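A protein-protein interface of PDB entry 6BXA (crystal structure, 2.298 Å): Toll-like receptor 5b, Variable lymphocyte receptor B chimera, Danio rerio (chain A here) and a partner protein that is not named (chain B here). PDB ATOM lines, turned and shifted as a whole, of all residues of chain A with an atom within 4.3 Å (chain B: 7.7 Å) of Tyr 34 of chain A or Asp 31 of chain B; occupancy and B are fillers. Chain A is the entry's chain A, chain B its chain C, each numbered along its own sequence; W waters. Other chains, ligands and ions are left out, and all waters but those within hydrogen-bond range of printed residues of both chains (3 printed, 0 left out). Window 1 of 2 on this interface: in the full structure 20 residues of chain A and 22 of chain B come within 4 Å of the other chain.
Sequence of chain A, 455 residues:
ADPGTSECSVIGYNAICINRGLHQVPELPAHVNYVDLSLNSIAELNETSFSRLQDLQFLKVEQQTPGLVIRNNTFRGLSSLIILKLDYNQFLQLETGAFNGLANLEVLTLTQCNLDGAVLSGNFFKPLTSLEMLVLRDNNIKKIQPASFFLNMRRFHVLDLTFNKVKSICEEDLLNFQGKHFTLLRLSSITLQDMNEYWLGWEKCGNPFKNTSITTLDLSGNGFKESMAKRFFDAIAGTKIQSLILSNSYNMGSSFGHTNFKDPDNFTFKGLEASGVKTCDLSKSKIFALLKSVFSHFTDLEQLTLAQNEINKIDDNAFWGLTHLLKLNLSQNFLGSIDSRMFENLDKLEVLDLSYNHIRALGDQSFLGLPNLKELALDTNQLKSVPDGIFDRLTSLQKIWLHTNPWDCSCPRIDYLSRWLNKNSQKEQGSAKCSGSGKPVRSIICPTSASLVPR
Of chain B, only Thr 29 (3.6 Å) and Asp 31 (3.8 Å) come within 4 Å of Tyr 34 of chain A.
Of the printed residues of chain A, Ser 26 of chain B touches Asn 33 and Phe 58.
Of the printed residues of chain B, Asn 33 of chain A touches Ser 26.
Of the printed residues of chain B, Phe 58 of chain A touches Ser 26 and Asp 31.
Thr 48 of chain B touches none of the printed residues of chain A.
The nearest printed residue of chain A that does not touch Asp 31 of chain B is Asp 36 of chain A (5.3 Å).
The nearest printed residue of chain A that does not touch Ser 26 of chain B is Asn 14 of chain A (4.1 Å).
OG1 of Thr 28 of chain B sits at hydrogen-bond distance from ND2 of Asn 14 of chain A, 3.1 Å away.
OD1 of Asn 14 of chain A sits at hydrogen-bond distance from OG1 of Thr 29 of chain B (2.6 Å).
The side-chain amino group (NZ) of Lys 60 of chain A lies within salt-bridge range of the side-chain carboxylate (OD2) of Asp 31 of chain B (2.9 Å).
NZ of Lys 60 of chain A is in hydrogen-bond range of OG of Ser 33 of chain B.
The side-chain amino group (NZ) of Lys 85 of chain A is in salt-bridge range of the side-chain carboxylate (OD1) of Asp 31 of chain B (3.0 Å).
Water W3 bridges O of Ser 33 of chain B and NZ of Lys 85 of chain A.
Water W1 lies within hydrogen-bond range of OH of Tyr 78 of chain B (2.7 Å), OD2 of Asp 36 of chain A (2.9 Å) and NZ of Lys 60 of chain A (2.9 Å).
Water W2 lies within hydrogen-bond range of OD2 of Asp 31 of chain B and OH of Tyr 34 of chain A.
Asn 14 of chain A touches Val 50 of chain B (ND2 to CG2, 3.9 Å).
CG1 of Ile 16 of chain A touches CD1 of Ile 74 of chain B, at 3.4 Å.
OD2 of Asp 31 of chain B touches OH of Tyr 34 of chain A, 3.8 Å away.
CZ of Phe 58 of chain A touches CB of Asp 31 of chain B, 3.8 Å away.
Printed residues of chain B that touch a printed residue of chain A: Ser 26, Thr 28, Thr 29, Asp 31, Ser 33, Val 50 and Ile 74.
Hydrophobic or aromatic side chains of chain B within 4 Å of the printed part of chain A: Val 50 and Ile 74.
Along chain B the printed residues that touch a printed residue of chain A span positions 26 to 74.
Of the 12 printed residues of chain A, 7 touch a printed residue of chain B.
Among the printed residues, Asp or Glu carboxylates within 4 Å of a Lys or Arg side-chain nitrogen of the other chain: Lys 60 of chain A with Asp 31 of chain B and Lys 85 of chain A with Asp 31 of chain B.
O of Tyr 34 of chain A is in hydrogen-bond range of N of Ala 15 of chain A (2.8 Å).
OD1 of Asp 31 of chain B sits at hydrogen-bond distance from OG of Ser 33 of chain B (2.5 Å).
SG of Cys 19 of chain B is disulfide-bonded to SG of Cys 25 of chain B, at 2.0 Å.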
ATOM      1  N   TYR A  13       0.943  -7.464   3.284  1.00  0.00           N
ATOM      2  CA  TYR A  13       0.980  -8.171   2.013  1.00  0.00           C
ATOM      3  C   TYR A  13       0.075  -7.517   0.969  1.00  0.00           C
ATOM      4  O   TYR A  13      -0.075  -8.036  -0.139  1.00  0.00           O
ATOM      5  CB  TYR A  13       0.585  -9.637   2.210  1.00  0.00           C
ATOM      6  CG  TYR A  13       1.528 -10.401   3.105  1.00  0.00           C
ATOM      7  CD1 TYR A  13       1.343 -10.422   4.484  1.00  0.00           C
ATOM      8  CD2 TYR A  13       2.612 -11.094   2.578  1.00  0.00           C
ATOM      9  CE1 TYR A  13       2.207 -11.116   5.312  1.00  0.00           C
ATOM     10  CE2 TYR A  13       3.485 -11.792   3.401  1.00  0.00           C
ATOM     11  CZ  TYR A  13       3.275 -11.799   4.766  1.00  0.00           C
ATOM     12  OH  TYR A  13       4.134 -12.489   5.594  1.00  0.00           O
ATOM     13  N   ASN A  14      -0.506  -6.372   1.322  1.00  0.00           N
ATOM     14  CA  ASN A  14      -1.412  -5.646   0.434  1.00  0.00           C
ATOM     15  C   ASN A  14      -0.728  -4.471  -0.240  1.00  0.00           C
ATOM     16  O   ASN A  14      -0.067  -3.670   0.424  1.00  0.00           O
ATOM     17  CB  ASN A  14      -2.616  -5.123   1.203  1.00  0.00           C
ATOM     18  CG  ASN A  14      -3.360  -6.210   1.917  1.00  0.00           C
ATOM     19  OD1 ASN A  14      -3.610  -7.273   1.357  1.00  0.00           O
ATOM     20  ND2 ASN A  14      -3.710  -5.964   3.171  1.00  0.00           N
ATOM     21  N   ALA A  15      -0.894  -4.361  -1.556  1.00  0.00           N
ATOM     22  CA  ALA A  15      -0.381  -3.208  -2.287  1.00  0.00           C
ATOM     23  C   ALA A  15      -1.524  -2.485  -2.973  1.00  0.00           C
ATOM     24  O   ALA A  15      -2.184  -3.036  -3.856  1.00  0.00           O
ATOM     25  CB  ALA A  15       0.671  -3.628  -3.300  1.00  0.00           C
ATOM     26  N   ILE A  16      -1.762  -1.249  -2.559  1.00  0.00           N
ATOM     27  CA  ILE A  16      -2.837  -0.454  -3.134  1.00  0.00           C
ATOM     28  C   ILE A  16      -2.275   0.571  -4.103  1.00  0.00           C
ATOM     29  O   ILE A  16      -1.564   1.498  -3.709  1.00  0.00           O
ATOM     30  CB  ILE A  16      -3.645   0.249  -2.043  1.00  0.00           C
ATOM     31  CG1 ILE A  16      -4.086  -0.776  -0.997  1.00  0.00           C
ATOM     32  CG2 ILE A  16      -4.832   0.988  -2.638  1.00  0.00           C
ATOM     33  CD1 ILE A  16      -4.907  -1.909  -1.537  1.00  0.00           C
ATOM     34  N   VAL A  32       4.222  -9.555  -1.611  1.00  0.00           N
ATOM     35  CA  VAL A  32       2.815  -9.148  -1.521  1.00  0.00           C
ATOM     36  C   VAL A  32       1.899 -10.141  -2.249  1.00  0.00           C
ATOM     37  O   VAL A  32       2.261 -10.664  -3.299  1.00  0.00           O
ATOM     38  CB  VAL A  32       2.598  -7.717  -2.093  1.00  0.00           C
ATOM     39  CG1 VAL A  32       3.408  -6.702  -1.291  1.00  0.00           C
ATOM     40  CG2 VAL A  32       2.958  -7.652  -3.571  1.00  0.00           C
ATOM     41  N   ASN A  33       0.727 -10.419  -1.693  1.00  0.00           N
ATOM     42  CA  ASN A  33      -0.160 -11.366  -2.354  1.00  0.00           C
ATOM     43  C   ASN A  33      -1.501 -10.758  -2.774  1.00  0.00           C
ATOM     44  O   ASN A  33      -2.301 -11.405  -3.451  1.00  0.00           O
ATOM     45  CB  ASN A  33      -0.391 -12.584  -1.461  1.00  0.00           C
ATOM     46  CG  ASN A  33      -0.854 -12.214  -0.071  1.00  0.00           C
ATOM     47  OD1 ASN A  33      -1.740 -11.375   0.104  1.00  0.00           O
ATOM     48  ND2 ASN A  33      -0.245 -12.835   0.935  1.00  0.00           N
ATOM     49  N   TYR A  34      -1.737  -9.512  -2.377  1.00  0.00           N
ATOM     50  CA  TYR A  34      -2.904  -8.769  -2.842  1.00  0.00           C
ATOM     51  C   TYR A  34      -2.457  -7.463  -3.472  1.00  0.00           C
ATOM     52  O   TYR A  34      -1.810  -6.640  -2.818  1.00  0.00           O
ATOM     53  CB  TYR A  34      -3.869  -8.471  -1.697  1.00  0.00           C
ATOM     54  CG  TYR A  34      -5.017  -7.580  -2.120  1.00  0.00           C
ATOM     55  CD1 TYR A  34      -6.129  -8.109  -2.769  1.00  0.00           C
ATOM     56  CD2 TYR A  34      -4.980  -6.208  -1.903  1.00  0.00           C
ATOM     57  CE1 TYR A  34      -7.175  -7.303  -3.167  1.00  0.00           C
ATOM     58  CE2 TYR A  34      -6.028  -5.390  -2.301  1.00  0.00           C
ATOM     59  CZ  TYR A  34      -7.122  -5.945  -2.934  1.00  0.00           C
ATOM     60  OH  TYR A  34      -8.167  -5.138  -3.337  1.00  0.00           O
ATOM     61  N   VAL A  35      -2.819  -7.258  -4.733  1.00  0.00           N
ATOM     62  CA  VAL A  35      -2.449  -6.030  -5.435  1.00  0.00           C
ATOM     63  C   VAL A  35      -3.657  -5.454  -6.178  1.00  0.00           C
ATOM     64  O   VAL A  35      -4.343  -6.159  -6.919  1.00  0.00           O
ATOM     65  CB  VAL A  35      -1.272  -6.270  -6.432  1.00  0.00           C
ATOM     66  CG1 VAL A  35      -0.988  -5.026  -7.246  1.00  0.00           C
ATOM     67  CG2 VAL A  35      -0.028  -6.670  -5.682  1.00  0.00           C
ATOM     68  N   ASP A  36      -3.935  -4.177  -5.945  1.00  0.00           N
ATOM     69  CA  ASP A  36      -4.998  -3.480  -6.651  1.00  0.00           C
ATOM     70  C   ASP A  36      -4.416  -2.403  -7.553  1.00  0.00           C
ATOM     71  O   ASP A  36      -3.924  -1.385  -7.061  1.00  0.00           O
ATOM     72  CB  ASP A  36      -5.985  -2.859  -5.667  1.00  0.00           C
ATOM     73  CG  ASP A  36      -7.251  -2.358  -6.343  1.00  0.00           C
ATOM     74  OD1 ASP A  36      -7.290  -2.297  -7.592  1.00  0.00           O
ATOM     75  OD2 ASP A  36      -8.211  -2.021  -5.615  1.00  0.00           O
ATOM     76  N   PHE A  58      -4.408 -12.535  -5.142  1.00  0.00           N
ATOM     77  CA  PHE A  58      -5.564 -11.689  -5.437  1.00  0.00           C
ATOM     78  C   PHE A  58      -5.086 -10.440  -6.193  1.00  0.00           C
ATOM     79  O   PHE A  58      -4.332  -9.620  -5.660  1.00  0.00           O
ATOM     80  CB  PHE A  58      -6.282 -11.361  -4.121  1.00  0.00           C
ATOM     81  CG  PHE A  58      -7.633 -10.702  -4.275  1.00  0.00           C
ATOM     82  CD1 PHE A  58      -8.068 -10.195  -5.492  1.00  0.00           C
ATOM     83  CD2 PHE A  58      -8.503 -10.652  -3.193  1.00  0.00           C
ATOM     84  CE1 PHE A  58      -9.308  -9.601  -5.610  1.00  0.00           C
ATOM     85  CE2 PHE A  58      -9.758 -10.069  -3.316  1.00  0.00           C
ATOM     86  CZ  PHE A  58     -10.153  -9.543  -4.525  1.00  0.00           C
ATOM     87  N   LYS A  60      -6.316  -7.220  -8.883  1.00  0.00           N
ATOM     88  CA  LYS A  60      -7.329  -6.412  -9.552  1.00  0.00           C
ATOM     89  C   LYS A  60      -6.624  -5.460 -10.503  1.00  0.00           C
ATOM     90  O   LYS A  60      -5.701  -4.741 -10.091  1.00  0.00           O
ATOM     91  CB  LYS A  60      -8.164  -5.611  -8.546  1.00  0.00           C
ATOM     92  CG  LYS A  60      -8.932  -6.444  -7.529  1.00  0.00           C
ATOM     93  CD  LYS A  60      -9.645  -5.555  -6.500  1.00  0.00           C
ATOM     94  CE  LYS A  60     -10.611  -4.586  -7.170  1.00  0.00           C
ATOM     95  NZ  LYS A  60     -11.450  -3.805  -6.208  1.00  0.00           N
ATOM     96  N   LYS A  85      -9.529 -10.064 -11.110  1.00  0.00           N
ATOM     97  CA  LYS A  85     -10.622  -9.180 -11.496  1.00  0.00           C
ATOM     98  C   LYS A  85     -10.146  -8.166 -12.522  1.00  0.00           C
ATOM     99  O   LYS A  85      -9.198  -7.412 -12.262  1.00  0.00           O
ATOM    100  CB  LYS A  85     -11.207  -8.470 -10.279  1.00  0.00           C
ATOM    101  CG  LYS A  85     -11.854  -9.419  -9.301  1.00  0.00           C
ATOM    102  CD  LYS A  85     -12.485  -8.702  -8.133  1.00  0.00           C
ATOM    103  CE  LYS A  85     -13.580  -9.556  -7.528  1.00  0.00           C
ATOM    104  NZ  LYS A  85     -14.126  -8.942  -6.274  1.00  0.00           N
ATOM    105  N   CYS B  19     -15.286 -14.666   6.259  1.00  0.00           N
ATOM    106  CA  CYS B  19     -15.499 -13.616   5.270  1.00  0.00           C
ATOM    107  C   CYS B  19     -16.984 -13.448   4.983  1.00  0.00           C
ATOM    108  O   CYS B  19     -17.700 -14.437   4.878  1.00  0.00           O
ATOM    109  CB  CYS B  19     -14.739 -13.947   3.982  1.00  0.00           C
ATOM    110  SG  CYS B  19     -14.734 -12.656   2.718  1.00  0.00           S
ATOM    111  N   PRO B  20     -17.456 -12.195   4.880  1.00  0.00           N
ATOM    112  CA  PRO B  20     -18.852 -11.920   4.521  1.00  0.00           C
ATOM    113  C   PRO B  20     -19.253 -12.602   3.207  1.00  0.00           C
ATOM    114  O   PRO B  20     -18.411 -12.757   2.322  1.00  0.00           O
ATOM    115  CB  PRO B  20     -18.885 -10.398   4.383  1.00  0.00           C
ATOM    116  CG  PRO B  20     -17.808  -9.928   5.293  1.00  0.00           C
ATOM    117  CD  PRO B  20     -16.718 -10.958   5.189  1.00  0.00           C
ATOM    118  N   GLN B  22     -21.030 -11.927   0.384  1.00  0.00           N
ATOM    119  CA  GLN B  22     -20.875 -11.300  -0.922  1.00  0.00           C
ATOM    120  C   GLN B  22     -19.428 -10.877  -1.197  1.00  0.00           C
ATOM    121  O   GLN B  22     -19.127 -10.335  -2.258  1.00  0.00           O
ATOM    122  CB  GLN B  22     -21.785 -10.077  -1.045  1.00  0.00           C
ATOM    123  CG  GLN B  22     -23.213 -10.272  -0.554  1.00  0.00           C
ATOM    124  CD  GLN B  22     -23.389  -9.881   0.911  1.00  0.00           C
ATOM    125  OE1 GLN B  22     -22.441  -9.929   1.702  1.00  0.00           O
ATOM    126  NE2 GLN B  22     -24.603  -9.472   1.271  1.00  0.00           N
ATOM    127  N   CYS B  23     -18.541 -11.117  -0.239  1.00  0.00           N
ATOM    128  CA  CYS B  23     -17.195 -10.569  -0.308  1.00  0.00           C
ATOM    129  C   CYS B  23     -16.101 -11.614  -0.559  1.00  0.00           C
ATOM    130  O   CYS B  23     -16.309 -12.813  -0.376  1.00  0.00           O
ATOM    131  CB  CYS B  23     -16.890  -9.801   0.986  1.00  0.00           C
ATOM    132  SG  CYS B  23     -18.001  -8.391   1.294  1.00  0.00           S
ATOM    133  N   SER B  24     -14.934 -11.131  -0.979  1.00  0.00           N
ATOM    134  CA  SER B  24     -13.755 -11.963  -1.192  1.00  0.00           C
ATOM    135  C   SER B  24     -12.640 -11.483  -0.266  1.00  0.00           C
ATOM    136  O   SER B  24     -12.333 -10.289  -0.225  1.00  0.00           O
ATOM    137  CB  SER B  24     -13.294 -11.902  -2.650  1.00  0.00           C
ATOM    138  OG  SER B  24     -14.245 -12.488  -3.522  1.00  0.00           O
ATOM    139  N   CYS B  25     -12.035 -12.407   0.477  1.00  0.00           N
ATOM    140  CA  CYS B  25     -11.058 -12.032   1.484  1.00  0.00           C
ATOM    141  C   CYS B  25      -9.682 -12.610   1.187  1.00  0.00           C
ATOM    142  O   CYS B  25      -9.553 -13.728   0.683  1.00  0.00           O
ATOM    143  CB  CYS B  25     -11.512 -12.484   2.877  1.00  0.00           C
ATOM    144  SG  CYS B  25     -13.066 -11.756   3.461  1.00  0.00           S
ATOM    145  N   SER B  26      -8.658 -11.834   1.521  1.00  0.00           N
ATOM    146  CA  SER B  26      -7.278 -12.266   1.393  1.00  0.00           C
ATOM    147  C   SER B  26      -6.434 -11.516   2.399  1.00  0.00           C
ATOM    148  O   SER B  26      -6.262 -10.303   2.299  1.00  0.00           O
ATOM    149  CB  SER B  26      -6.748 -12.024  -0.014  1.00  0.00           C
ATOM    150  OG  SER B  26      -5.367 -12.352  -0.088  1.00  0.00           O
ATOM    151  N   GLY B  27      -5.916 -12.243   3.375  1.00  0.00           N
ATOM    152  CA  GLY B  27      -5.168 -11.623   4.448  1.00  0.00           C
ATOM    153  C   GLY B  27      -6.067 -10.684   5.225  1.00  0.00           C
ATOM    154  O   GLY B  27      -7.131 -11.085   5.698  1.00  0.00           O
ATOM    155  N   THR B  28      -5.649  -9.426   5.325  1.00  0.00           N
ATOM    156  CA  THR B  28      -6.426  -8.408   6.023  1.00  0.00           C
ATOM    157  C   THR B  28      -7.255  -7.574   5.054  1.00  0.00           C
ATOM    158  O   THR B  28      -7.715  -6.482   5.393  1.00  0.00           O
ATOM    159  CB  THR B  28      -5.518  -7.471   6.838  1.00  0.00           C
ATOM    160  OG1 THR B  28      -4.493  -6.945   5.983  1.00  0.00           O
ATOM    161  CG2 THR B  28      -4.869  -8.225   7.975  1.00  0.00           C
ATOM    162  N   THR B  29      -7.444  -8.102   3.850  1.00  0.00           N
ATOM    163  CA  THR B  29      -8.216  -7.421   2.824  1.00  0.00           C
ATOM    164  C   THR B  29      -9.595  -8.046   2.631  1.00  0.00           C
ATOM    165  O   THR B  29      -9.731  -9.267   2.499  1.00  0.00           O
ATOM    166  CB  THR B  29      -7.475  -7.430   1.475  1.00  0.00           C
ATOM    167  OG1 THR B  29      -6.202  -6.797   1.634  1.00  0.00           O
ATOM    168  CG2 THR B  29      -8.275  -6.704   0.401  1.00  0.00           C
ATOM    169  N   VAL B  30     -10.615  -7.193   2.612  1.00  0.00           N
ATOM    170  CA  VAL B  30     -11.972  -7.610   2.308  1.00  0.00           C
ATOM    171  C   VAL B  30     -12.511  -6.802   1.133  1.00  0.00           C
ATOM    172  O   VAL B  30     -12.736  -5.592   1.250  1.00  0.00           O
ATOM    173  CB  VAL B  30     -12.911  -7.444   3.515  1.00  0.00           C
ATOM    174  CG1 VAL B  30     -14.347  -7.748   3.117  1.00  0.00           C
ATOM    175  CG2 VAL B  30     -12.467  -8.343   4.658  1.00  0.00           C
ATOM    176  N   ASP B  31     -12.709  -7.476   0.003  1.00  0.00           N
ATOM    177  CA  ASP B  31     -13.182  -6.818  -1.202  1.00  0.00           C
ATOM    178  C   ASP B  31     -14.634  -7.202  -1.483  1.00  0.00           C
ATOM    179  O   ASP B  31     -14.938  -8.360  -1.785  1.00  0.00           O
ATOM    180  CB  ASP B  31     -12.299  -7.185  -2.388  1.00  0.00           C
ATOM    181  CG  ASP B  31     -12.627  -6.380  -3.626  1.00  0.00           C
ATOM    182  OD1 ASP B  31     -13.547  -6.760  -4.367  1.00  0.00           O
ATOM    183  OD2 ASP B  31     -11.944  -5.348  -3.851  1.00  0.00           O
ATOM    184  N   CYS B  32     -15.520  -6.218  -1.369  1.00  0.00           N
ATOM    185  CA  CYS B  32     -16.946  -6.398  -1.597  1.00  0.00           C
ATOM    186  C   CYS B  32     -17.381  -5.581  -2.800  1.00  0.00           C
ATOM    187  O   CYS B  32     -18.542  -5.185  -2.918  1.00  0.00           O
ATOM    188  CB  CYS B  32     -17.750  -5.972  -0.372  1.00  0.00           C
ATOM    189  SG  CYS B  32     -17.103  -6.553   1.203  1.00  0.00           S
ATOM    190  N   SER B  33     -16.430  -5.339  -3.688  1.00  0.00           N
ATOM    191  CA  SER B  33     -16.634  -4.482  -4.842  1.00  0.00           C
ATOM    192  C   SER B  33     -17.377  -5.187  -5.960  1.00  0.00           C
ATOM    193  O   SER B  33     -17.202  -6.387  -6.163  1.00  0.00           O
ATOM    194  CB  SER B  33     -15.296  -4.008  -5.377  1.00  0.00           C
ATOM    195  OG  SER B  33     -14.608  -5.126  -5.908  1.00  0.00           O
ATOM    196  N   GLY B  34     -18.185  -4.419  -6.688  1.00  0.00           N
ATOM    197  CA  GLY B  34     -18.890  -4.913  -7.855  1.00  0.00           C
ATOM    198  C   GLY B  34     -19.903  -5.998  -7.556  1.00  0.00           C
ATOM    199  O   GLY B  34     -20.068  -6.923  -8.345  1.00  0.00           O
ATOM    200  N   LYS B  35     -20.589  -5.894  -6.424  1.00  0.00           N
ATOM    201  CA  LYS B  35     -21.541  -6.925  -6.048  1.00  0.00           C
ATOM    202  C   LYS B  35     -22.960  -6.404  -5.946  1.00  0.00           C
ATOM    203  O   LYS B  35     -23.801  -7.043  -5.313  1.00  0.00           O
ATOM    204  CB  LYS B  35     -21.143  -7.554  -4.710  1.00  0.00           C
ATOM    205  CG  LYS B  35     -19.933  -8.465  -4.770  1.00  0.00           C
ATOM    206  CD  LYS B  35     -20.249  -9.689  -5.606  1.00  0.00           C
ATOM    207  CE  LYS B  35     -19.076 -10.641  -5.675  1.00  0.00           C
ATOM    208  NZ  LYS B  35     -19.575 -11.987  -6.089  1.00  0.00           N
ATOM    209  N   LEU B  37     -24.154  -4.217  -4.151  1.00  0.00           N
ATOM    210  CA  LEU B  37     -24.535  -4.045  -2.761  1.00  0.00           C
ATOM    211  C   LEU B  37     -25.309  -2.747  -2.592  1.00  0.00           C
ATOM    212  O   LEU B  37     -24.963  -1.732  -3.180  1.00  0.00           O
ATOM    213  CB  LEU B  37     -23.304  -4.036  -1.862  1.00  0.00           C
ATOM    214  CG  LEU B  37     -22.471  -5.309  -1.823  1.00  0.00           C
ATOM    215  CD1 LEU B  37     -21.311  -5.099  -0.890  1.00  0.00           C
ATOM    216  CD2 LEU B  37     -23.328  -6.470  -1.357  1.00  0.00           C
ATOM    217  N   PRO B  41     -21.930  -4.749   4.034  1.00  0.00           N
ATOM    218  CA  PRO B  41     -22.117  -6.104   4.562  1.00  0.00           C
ATOM    219  C   PRO B  41     -21.803  -6.170   6.046  1.00  0.00           C
ATOM    220  O   PRO B  41     -20.951  -5.424   6.536  1.00  0.00           O
ATOM    221  CB  PRO B  41     -21.120  -6.942   3.755  1.00  0.00           C
ATOM    222  CG  PRO B  41     -20.875  -6.158   2.519  1.00  0.00           C
ATOM    223  CD  PRO B  41     -20.936  -4.718   2.945  1.00  0.00           C
ATOM    224  N   THR B  48      -9.735  -6.273   9.939  1.00  0.00           N
ATOM    225  CA  THR B  48      -9.690  -5.763   8.576  1.00  0.00           C
ATOM    226  C   THR B  48      -8.893  -4.469   8.465  1.00  0.00           C
ATOM    227  O   THR B  48      -9.163  -3.492   9.167  1.00  0.00           O
ATOM    228  CB  THR B  48     -11.103  -5.546   8.024  1.00  0.00           C
ATOM    229  OG1 THR B  48     -11.804  -6.797   8.039  1.00  0.00           O
ATOM    230  CG2 THR B  48     -11.044  -5.023   6.594  1.00  0.00           C
ATOM    231  N   VAL B  50      -7.933  -3.386   5.071  1.00  0.00           N
ATOM    232  CA  VAL B  50      -8.356  -2.869   3.773  1.00  0.00           C
ATOM    233  C   VAL B  50      -9.781  -3.324   3.462  1.00  0.00           C
ATOM    234  O   VAL B  50     -10.063  -4.523   3.427  1.00  0.00           O
ATOM    235  CB  VAL B  50      -7.420  -3.330   2.634  1.00  0.00           C
ATOM    236  CG1 VAL B  50      -7.928  -2.827   1.285  1.00  0.00           C
ATOM    237  CG2 VAL B  50      -6.001  -2.860   2.890  1.00  0.00           C
ATOM    238  N   LEU B  51     -10.673  -2.367   3.239  1.00  0.00           N
ATOM    239  CA  LEU B  51     -12.064  -2.674   2.939  1.00  0.00           C
ATOM    240  C   LEU B  51     -12.494  -2.024   1.627  1.00  0.00           C
ATOM    241  O   LEU B  51     -12.464  -0.799   1.487  1.00  0.00           O
ATOM    242  CB  LEU B  51     -12.968  -2.228   4.092  1.00  0.00           C
ATOM    243  CG  LEU B  51     -14.478  -2.438   3.911  1.00  0.00           C
ATOM    244  CD1 LEU B  51     -14.837  -3.911   3.671  1.00  0.00           C
ATOM    245  CD2 LEU B  51     -15.249  -1.873   5.115  1.00  0.00           C
ATOM    246  N   GLY B  52     -12.865  -2.856   0.660  1.00  0.00           N
ATOM    247  CA  GLY B  52     -13.272  -2.376  -0.651  1.00  0.00           C
ATOM    248  C   GLY B  52     -14.765  -2.492  -0.885  1.00  0.00           C
ATOM    249  O   GLY B  52     -15.330  -3.592  -0.888  1.00  0.00           O
ATOM    250  N   LEU B  53     -15.410  -1.353  -1.095  1.00  0.00           N
ATOM    251  CA  LEU B  53     -16.845  -1.330  -1.314  1.00  0.00           C
ATOM    252  C   LEU B  53     -17.176  -0.594  -2.605  1.00  0.00           C
ATOM    253  O   LEU B  53     -18.307  -0.151  -2.794  1.00  0.00           O
ATOM    254  CB  LEU B  53     -17.558  -0.675  -0.126  1.00  0.00           C
ATOM    255  CG  LEU B  53     -17.451  -1.411   1.210  1.00  0.00           C
ATOM    256  CD1 LEU B  53     -17.771  -0.499   2.385  1.00  0.00           C
ATOM    257  CD2 LEU B  53     -18.386  -2.600   1.208  1.00  0.00           C
ATOM    258  N   SER B  54     -16.189  -0.461  -3.488  1.00  0.00           N
ATOM    259  CA  SER B  54     -16.380   0.302  -4.718  1.00  0.00           C
ATOM    260  C   SER B  54     -17.327  -0.376  -5.715  1.00  0.00           C
ATOM    261  O   SER B  54     -17.581  -1.587  -5.634  1.00  0.00           O
ATOM    262  CB  SER B  54     -15.037   0.559  -5.391  1.00  0.00           C
ATOM    263  OG  SER B  54     -14.512  -0.639  -5.921  1.00  0.00           O
ATOM    264  N   ASN B  56     -20.637  -0.289  -6.320  1.00  0.00           N
ATOM    265  CA  ASN B  56     -21.861  -0.896  -5.837  1.00  0.00           C
ATOM    266  C   ASN B  56     -23.003   0.098  -5.980  1.00  0.00           C
ATOM    267  O   ASN B  56     -22.887   1.069  -6.717  1.00  0.00           O
ATOM    268  CB  ASN B  56     -21.716  -1.346  -4.383  1.00  0.00           C
ATOM    269  CG  ASN B  56     -20.939  -2.636  -4.251  1.00  0.00           C
ATOM    270  OD1 ASN B  56     -21.331  -3.659  -4.805  1.00  0.00           O
ATOM    271  ND2 ASN B  56     -19.830  -2.597  -3.520  1.00  0.00           N
ATOM    272  N   ILE B  74      -7.424   1.462   4.958  1.00  0.00           N
ATOM    273  CA  ILE B  74      -7.870   1.817   3.618  1.00  0.00           C
ATOM    274  C   ILE B  74      -9.354   1.539   3.443  1.00  0.00           C
ATOM    275  O   ILE B  74      -9.806   0.408   3.617  1.00  0.00           O
ATOM    276  CB  ILE B  74      -7.078   1.062   2.541  1.00  0.00           C
ATOM    277  CG1 ILE B  74      -5.621   1.521   2.553  1.00  0.00           C
ATOM    278  CG2 ILE B  74      -7.651   1.332   1.162  1.00  0.00           C
ATOM    279  CD1 ILE B  74      -4.678   0.457   2.153  1.00  0.00           C
ATOM    280  N   VAL B  76     -12.412   2.062   0.659  1.00  0.00           N
ATOM    281  CA  VAL B  76     -12.653   2.381  -0.744  1.00  0.00           C
ATOM    282  C   VAL B  76     -14.151   2.394  -1.070  1.00  0.00           C
ATOM    283  O   VAL B  76     -14.823   1.355  -1.040  1.00  0.00           O
ATOM    284  CB  VAL B  76     -11.913   1.384  -1.668  1.00  0.00           C
ATOM    285  CG1 VAL B  76     -11.982   1.841  -3.090  1.00  0.00           C
ATOM    286  CG2 VAL B  76     -10.455   1.240  -1.238  1.00  0.00           C
ATOM    287  N   TYR B  78     -15.491   4.460  -3.867  1.00  0.00           N
ATOM    288  CA  TYR B  78     -15.732   5.174  -5.108  1.00  0.00           C
ATOM    289  C   TYR B  78     -16.775   4.427  -5.941  1.00  0.00           C
ATOM    290  O   TYR B  78     -16.977   3.222  -5.770  1.00  0.00           O
ATOM    291  CB  TYR B  78     -14.428   5.410  -5.904  1.00  0.00           C
ATOM    292  CG  TYR B  78     -13.714   4.192  -6.451  1.00  0.00           C
ATOM    293  CD1 TYR B  78     -14.193   3.526  -7.567  1.00  0.00           C
ATOM    294  CD2 TYR B  78     -12.527   3.744  -5.885  1.00  0.00           C
ATOM    295  CE1 TYR B  78     -13.540   2.426  -8.073  1.00  0.00           C
ATOM    296  CE2 TYR B  78     -11.863   2.640  -6.388  1.00  0.00           C
ATOM    297  CZ  TYR B  78     -12.378   1.989  -7.480  1.00  0.00           C
ATOM    298  OH  TYR B  78     -11.735   0.894  -7.985  1.00  0.00           O
HETATM  299  O   HOH W   1     -10.817  -0.931  -6.207  1.00  0.00           O
HETATM  300  O   HOH W   2     -10.464  -3.278  -2.787  1.00  0.00           O
HETATM  301  O   HOH W   3     -15.701  -7.375  -7.892  1.00  0.00           O
